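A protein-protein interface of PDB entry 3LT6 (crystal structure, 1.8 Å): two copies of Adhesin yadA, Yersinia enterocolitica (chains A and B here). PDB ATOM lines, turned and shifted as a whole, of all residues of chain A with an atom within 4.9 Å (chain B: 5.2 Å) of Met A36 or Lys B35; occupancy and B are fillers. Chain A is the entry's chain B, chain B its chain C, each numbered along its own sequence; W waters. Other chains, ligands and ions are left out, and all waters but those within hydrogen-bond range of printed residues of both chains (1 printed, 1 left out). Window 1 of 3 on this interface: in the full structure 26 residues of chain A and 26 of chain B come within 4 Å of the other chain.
Thr B32 touches its own counterpart, Thr A32.
Thr A32 touches Lys B35, but with the chains exchanged Lys A35 does not touch Thr B32 (8.3 Å).
Asp A33 touches Lys B35, but with the chains exchanged Lys A35 does not touch Asp B33 (11.3 Å).
Met B36 touches its own counterpart, Met A36.
9 positions are printed for both chains.
Of the 11 pairs that touch across the chains among the printed residues, 3 have their exchanged pair printed and touching as well.
Water W1 lies within hydrogen-bond range of OG1 of Thr A32 (2.6 Å) and OG1 of Thr B32 (3.0 Å).
Met A36 touches just these residues of chain B: Thr B32, Lys B35, Met B36 and Leu B39.
Lys B35 touches just these residues of chain A: Thr A32 (3.9 Å), Asp A33 (2.5 Å) and Met A36 (3.8 Å).
Of the printed residues of chain A, Thr B32 touches Thr A32 (3.1 Å) and Met A36 (3.9 Å).
Of the printed residues of chain B, Glu A40 touches Leu B39.
His A34 touches none of the printed residues of chain B.
His B34 touches none of the printed residues of chain A.
The nearest residue of chain A that does not touch Lys B35 is His A37 (4.6 Å).
The backbone carbonyl oxygen (O) of Asp A33 lies close to a ring nitrogen (ND1) of His A37.
OH of Tyr B31 is in hydrogen-bond range of NZ of Lys B35 (3.3 Å).
The side-chain hydroxyl of Thr B32 sits at hydrogen-bond distance from the side-chain hydroxyl of Thr A32 (3.1 Å).
OD1 of Asp A33 lies within hydrogen-bond range of OH of Tyr B31 (2.5 Å).
NZ of Lys B35 is in salt-bridge range of OD1 of Asp A33 (2.5 Å).
Of the 9 printed residues of chain A, 5 touch a printed residue of chain B.
Hydrophobic or aromatic side chains of chain A within 4 Å of the printed part of chain B: Met A36 and Leu A39.
Of the 10 printed residues of chain B, 5 touch a printed residue of chain A.
Hydrophobic or aromatic side chains of chain B that line the printed part of chain A: Tyr B31, Met B36 and Leu B39.
Among the printed residues, pairs that only touch across the chains: Met A36 with Leu B39 (3.1 Å), Leu A39 with Leu B39 (3.5 Å), Met A36 with Met B36 (3.8 Å), Met A36 with Lys B35 (3.8 Å), Thr A32 with Tyr B31 (3.9 Å), Thr A32 with Lys B35 (3.9 Å), Glu A40 with Leu B39 (3.9 Å) and Met A36 with Thr B32 (3.9 Å).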
ATOM      1  N   THR A  32       7.543  17.360  13.807  1.00  0.00           N
ATOM      2  CA  THR A  32       7.670  17.822  15.165  1.00  0.00           C
ATOM      3  C   THR A  32       9.043  17.291  15.573  1.00  0.00           C
ATOM      4  O   THR A  32       9.886  18.081  16.004  1.00  0.00           O
ATOM      5  CB  THR A  32       6.628  17.170  16.043  1.00  0.00           C
ATOM      6  OG1 THR A  32       5.312  17.666  15.630  1.00  0.00           O
ATOM      7  CG2 THR A  32       6.976  17.460  17.542  1.00  0.00           C
ATOM      8  N   ASP A  33       9.325  16.050  15.224  1.00  0.00           N
ATOM      9  CA  ASP A  33      10.707  15.498  15.576  1.00  0.00           C
ATOM     10  C   ASP A  33      11.861  16.259  14.955  1.00  0.00           C
ATOM     11  O   ASP A  33      12.880  16.503  15.645  1.00  0.00           O
ATOM     12  CB  ASP A  33      10.884  14.013  15.147  1.00  0.00           C
ATOM     13  CG  ASP A  33      10.287  13.021  16.152  1.00  0.00           C
ATOM     14  OD1 ASP A  33       9.994  13.412  17.328  1.00  0.00           O
ATOM     15  OD2 ASP A  33      10.103  11.834  15.774  1.00  0.00           O
ATOM     16  N   HIS A  34      11.753  16.590  13.674  1.00  0.00           N
ATOM     17  CA  HIS A  34      12.807  17.402  13.020  1.00  0.00           C
ATOM     18  C   HIS A  34      12.944  18.821  13.613  1.00  0.00           C
ATOM     19  O   HIS A  34      14.047  19.289  13.832  1.00  0.00           O
ATOM     20  CB  HIS A  34      12.713  17.381  11.490  1.00  0.00           C
ATOM     21  CG  HIS A  34      12.506  16.001  10.929  1.00  0.00           C
ATOM     22  ND1 HIS A  34      12.371  15.746   9.581  1.00  0.00           N
ATOM     23  CD2 HIS A  34      12.362  14.803  11.552  1.00  0.00           C
ATOM     24  CE1 HIS A  34      12.206  14.447   9.392  1.00  0.00           C
ATOM     25  NE2 HIS A  34      12.160  13.858  10.576  1.00  0.00           N
ATOM     26  N   LYS A  35      11.826  19.475  13.907  1.00  0.00           N
ATOM     27  CA  LYS A  35      11.899  20.821  14.476  1.00  0.00           C
ATOM     28  C   LYS A  35      12.476  20.806  15.896  1.00  0.00           C
ATOM     29  O   LYS A  35      13.270  21.719  16.248  1.00  0.00           O
ATOM     30  CB  LYS A  35      10.506  21.488  14.433  1.00  0.00           C
ATOM     31  CG  LYS A  35       9.851  21.627  13.107  1.00  0.00           C
ATOM     32  CD  LYS A  35      10.649  22.518  12.097  1.00  0.00           C
ATOM     33  CE  LYS A  35      10.140  23.951  12.133  1.00  0.00           C
ATOM     34  NZ  LYS A  35      10.270  24.659  10.834  1.00  0.00           N
ATOM     35  N   MET A  36      12.134  19.763  16.669  1.00  0.00           N
ATOM     36  CA  MET A  36      12.587  19.628  18.046  1.00  0.00           C
ATOM     37  C   MET A  36      14.073  19.242  18.050  1.00  0.00           C
ATOM     38  O   MET A  36      14.809  19.787  18.875  1.00  0.00           O
ATOM     39  CB  MET A  36      11.693  18.683  18.914  1.00  0.00           C
ATOM     40  CG  MET A  36      10.238  19.155  18.957  1.00  0.00           C
ATOM     41  SD  MET A  36       9.986  20.533  20.320  1.00  0.00           S
ATOM     42  CE  MET A  36       8.088  21.153  20.265  1.00  0.00           C
ATOM     43  N   HIS A  37      14.504  18.371  17.117  1.00  0.00           N
ATOM     44  CA  HIS A  37      15.941  17.996  16.965  1.00  0.00           C
ATOM     45  C   HIS A  37      16.828  19.210  16.692  1.00  0.00           C
ATOM     46  O   HIS A  37      17.941  19.270  17.214  1.00  0.00           O
ATOM     47  CB  HIS A  37      16.186  16.967  15.822  1.00  0.00           C
ATOM     48  CG  HIS A  37      15.651  15.579  16.081  1.00  0.00           C
ATOM     49  ND1 HIS A  37      15.507  14.639  15.074  1.00  0.00           N
ATOM     50  CD2 HIS A  37      15.252  14.959  17.219  1.00  0.00           C
ATOM     51  CE1 HIS A  37      15.033  13.510  15.577  1.00  0.00           C
ATOM     52  NE2 HIS A  37      14.873  13.675  16.878  1.00  0.00           N
ATOM     53  N   GLN A  38      16.358  20.148  15.857  1.00  0.00           N
ATOM     54  CA  GLN A  38      17.126  21.390  15.533  1.00  0.00           C
ATOM     55  C   GLN A  38      17.367  22.249  16.784  1.00  0.00           C
ATOM     56  O   GLN A  38      18.478  22.753  17.025  1.00  0.00           O
ATOM     57  CB  GLN A  38      16.407  22.224  14.454  1.00  0.00           C
ATOM     58  CG  GLN A  38      16.369  21.535  13.105  1.00  0.00           C
ATOM     59  CD  GLN A  38      15.673  22.376  12.062  1.00  0.00           C
ATOM     60  OE1 GLN A  38      14.536  22.802  12.255  1.00  0.00           O
ATOM     61  NE2 GLN A  38      16.332  22.597  10.946  1.00  0.00           N
ATOM     62  N   LEU A  39      16.315  22.400  17.584  1.00  0.00           N
ATOM     63  CA  LEU A  39      16.397  23.184  18.796  1.00  0.00           C
ATOM     64  C   LEU A  39      17.296  22.485  19.778  1.00  0.00           C
ATOM     65  O   LEU A  39      18.171  23.117  20.341  1.00  0.00           O
ATOM     66  CB  LEU A  39      15.017  23.339  19.432  1.00  0.00           C
ATOM     67  CG  LEU A  39      14.972  24.208  20.708  1.00  0.00           C
ATOM     68  CD1 LEU A  39      15.346  25.668  20.343  1.00  0.00           C
ATOM     69  CD2 LEU A  39      13.593  24.191  21.272  1.00  0.00           C
ATOM     70  N   GLU A  40      17.069  21.177  19.988  1.00  0.00           N
ATOM     71  CA  GLU A  40      17.948  20.360  20.853  1.00  0.00           C
ATOM     72  C   GLU A  40      19.396  20.542  20.516  1.00  0.00           C
ATOM     73  O   GLU A  40      20.212  20.652  21.404  1.00  0.00           O
ATOM     74  CB  GLU A  40      17.633  18.875  20.721  1.00  0.00           C
ATOM     75  CG  GLU A  40      16.536  18.356  21.667  1.00  0.00           C
ATOM     76  CD  GLU A  40      15.895  17.051  21.151  1.00  0.00           C
ATOM     77  OE1 GLU A  40      16.519  15.965  21.334  1.00  0.00           O
ATOM     78  OE2 GLU A  40      14.754  17.099  20.580  1.00  0.00           O
ATOM     79  N   TYR B  31       1.384  14.830  20.911  1.00  0.00           N
ATOM     80  CA  TYR B  31       2.855  14.428  20.797  1.00  0.00           C
ATOM     81  C   TYR B  31       3.722  15.705  20.883  1.00  0.00           C
ATOM     82  O   TYR B  31       4.779  15.701  21.560  1.00  0.00           O
ATOM     83  CB  TYR B  31       3.116  13.682  19.454  1.00  0.00           C
ATOM     84  CG  TYR B  31       4.582  13.276  19.265  1.00  0.00           C
ATOM     85  CD1 TYR B  31       5.064  12.126  19.862  1.00  0.00           C
ATOM     86  CD2 TYR B  31       5.423  14.001  18.404  1.00  0.00           C
ATOM     87  CE1 TYR B  31       6.362  11.684  19.667  1.00  0.00           C
ATOM     88  CE2 TYR B  31       6.781  13.634  18.242  1.00  0.00           C
ATOM     89  CZ  TYR B  31       7.242  12.453  18.905  1.00  0.00           C
ATOM     90  OH  TYR B  31       8.548  11.975  18.831  1.00  0.00           O
ATOM     91  N   THR B  32       3.328  16.726  20.138  1.00  0.00           N
ATOM     92  CA  THR B  32       3.920  18.028  20.190  1.00  0.00           C
ATOM     93  C   THR B  32       4.088  18.590  21.618  1.00  0.00           C
ATOM     94  O   THR B  32       5.129  19.169  21.958  1.00  0.00           O
ATOM     95  CB  THR B  32       3.218  19.063  19.242  1.00  0.00           C
ATOM     96  OG1 THR B  32       3.392  18.610  17.901  1.00  0.00           O
ATOM     97  CG2 THR B  32       3.973  20.397  19.467  1.00  0.00           C
ATOM     98  N   ASP B  33       3.029  18.473  22.415  1.00  0.00           N
ATOM     99  CA  ASP B  33       2.971  18.998  23.770  1.00  0.00           C
ATOM    100  C   ASP B  33       4.002  18.204  24.554  1.00  0.00           C
ATOM    101  O   ASP B  33       4.744  18.755  25.386  1.00  0.00           O
ATOM    102  CB  ASP B  33       1.533  18.794  24.253  1.00  0.00           C
ATOM    103  CG  ASP B  33       0.601  19.863  23.774  1.00  0.00           C
ATOM    104  OD1 ASP B  33       1.074  20.853  23.147  1.00  0.00           O
ATOM    105  OD2 ASP B  33      -0.638  19.623  23.860  1.00  0.00           O
ATOM    106  N   HIS B  34       4.068  16.915  24.242  1.00  0.00           N
ATOM    107  CA  HIS B  34       5.004  16.013  24.930  1.00  0.00           C
ATOM    108  C   HIS B  34       6.439  16.453  24.672  1.00  0.00           C
ATOM    109  O   HIS B  34       7.230  16.531  25.629  1.00  0.00           O
ATOM    110  CB  HIS B  34       4.810  14.565  24.493  1.00  0.00           C
ATOM    111  CG  HIS B  34       5.982  13.673  24.795  1.00  0.00           C
ATOM    112  ND1 HIS B  34       6.429  13.435  26.076  1.00  0.00           N
ATOM    113  CD2 HIS B  34       6.814  12.978  23.972  1.00  0.00           C
ATOM    114  CE1 HIS B  34       7.484  12.630  26.038  1.00  0.00           C
ATOM    115  NE2 HIS B  34       7.728  12.327  24.773  1.00  0.00           N
ATOM    116  N   LYS B  35       6.800  16.700  23.398  1.00  0.00           N
ATOM    117  CA  LYS B  35       8.172  17.175  23.071  1.00  0.00           C
ATOM    118  C   LYS B  35       8.495  18.590  23.587  1.00  0.00           C
ATOM    119  O   LYS B  35       9.644  18.887  23.940  1.00  0.00           O
ATOM    120  CB  LYS B  35       8.444  17.046  21.563  1.00  0.00           C
ATOM    121  CG  LYS B  35       7.959  15.761  20.910  1.00  0.00           C
ATOM    122  CD  LYS B  35       9.029  14.579  21.035  1.00  0.00           C
ATOM    123  CE  LYS B  35      10.369  15.077  20.379  1.00  0.00           C
ATOM    124  NZ  LYS B  35      11.048  14.060  19.470  1.00  0.00           N
ATOM    125  N   MET B  36       7.503  19.493  23.608  1.00  0.00           N
ATOM    126  CA  MET B  36       7.767  20.843  24.094  1.00  0.00           C
ATOM    127  C   MET B  36       8.013  20.839  25.621  1.00  0.00           C
ATOM    128  O   MET B  36       8.851  21.576  26.199  1.00  0.00           O
ATOM    129  CB  MET B  36       6.515  21.689  23.789  1.00  0.00           C
ATOM    130  CG  MET B  36       6.643  23.145  24.242  1.00  0.00           C
ATOM    131  SD  MET B  36       4.879  23.908  24.380  1.00  0.00           S
ATOM    132  CE  MET B  36       4.054  22.868  25.889  1.00  0.00           C
ATOM    133  N   HIS B  37       7.346  19.927  26.302  1.00  0.00           N
ATOM    134  CA  HIS B  37       7.600  19.722  27.723  1.00  0.00           C
ATOM    135  C   HIS B  37       9.024  19.291  27.949  1.00  0.00           C
ATOM    136  O   HIS B  37       9.658  19.775  28.883  1.00  0.00           O
ATOM    137  CB  HIS B  37       6.719  18.615  28.311  1.00  0.00           C
ATOM    138  CG  HIS B  37       5.288  18.998  28.477  1.00  0.00           C
ATOM    139  ND1 HIS B  37       4.380  18.171  29.127  1.00  0.00           N
ATOM    140  CD2 HIS B  37       4.609  20.126  28.169  1.00  0.00           C
ATOM    141  CE1 HIS B  37       3.192  18.747  29.148  1.00  0.00           C
ATOM    142  NE2 HIS B  37       3.295  19.925  28.558  1.00  0.00           N
ATOM    143  N   GLN B  38       9.551  18.459  27.070  1.00  0.00           N
ATOM    144  CA  GLN B  38      10.926  17.917  27.292  1.00  0.00           C
ATOM    145  C   GLN B  38      11.951  19.068  27.077  1.00  0.00           C
ATOM    146  O   GLN B  38      12.896  19.260  27.828  1.00  0.00           O
ATOM    147  CB  GLN B  38      11.228  16.710  26.399  1.00  0.00           C
ATOM    148  CG  GLN B  38      10.381  15.369  26.675  1.00  0.00           C
ATOM    149  CD  GLN B  38      10.646  14.349  25.575  1.00  0.00           C
ATOM    150  OE1 GLN B  38      10.728  14.696  24.398  1.00  0.00           O
ATOM    151  NE2 GLN B  38      10.825  13.091  25.957  1.00  0.00           N
ATOM    152  N   LEU B  39      11.714  19.883  26.056  1.00  0.00           N
ATOM    153  CA  LEU B  39      12.547  21.053  25.787  1.00  0.00           C
ATOM    154  C   LEU B  39      12.338  22.201  26.781  1.00  0.00           C
ATOM    155  O   LEU B  39      13.337  22.814  27.138  1.00  0.00           O
ATOM    156  CB  LEU B  39      12.340  21.497  24.361  1.00  0.00           C
ATOM    157  CG  LEU B  39      13.136  20.647  23.367  1.00  0.00           C
ATOM    158  CD1 LEU B  39      12.465  20.665  22.148  1.00  0.00           C
ATOM    159  CD2 LEU B  39      14.479  21.346  23.192  1.00  0.00           C
ATOM    160  N   GLU B  40      11.100  22.460  27.268  1.00  0.00           N
ATOM    161  CA  GLU B  40      10.931  23.277  28.443  1.00  0.00           C
ATOM    162  C   GLU B  40      11.747  22.883  29.683  1.00  0.00           C
ATOM    163  O   GLU B  40      12.484  23.728  30.233  1.00  0.00           O
ATOM    164  CB  GLU B  40       9.427  23.546  28.742  1.00  0.00           C
ATOM    165  CG  GLU B  40       8.905  24.635  27.767  1.00  0.00           C
ATOM    166  CD  GLU B  40       9.618  25.938  27.964  1.00  0.00           C
ATOM    167  OE1 GLU B  40       9.591  26.467  29.100  1.00  0.00           O
ATOM    168  OE2 GLU B  40      10.228  26.455  27.012  1.00  0.00           O
HETATM  169  O   HOH W   1       3.253  16.163  16.096  1.00  0.00           O
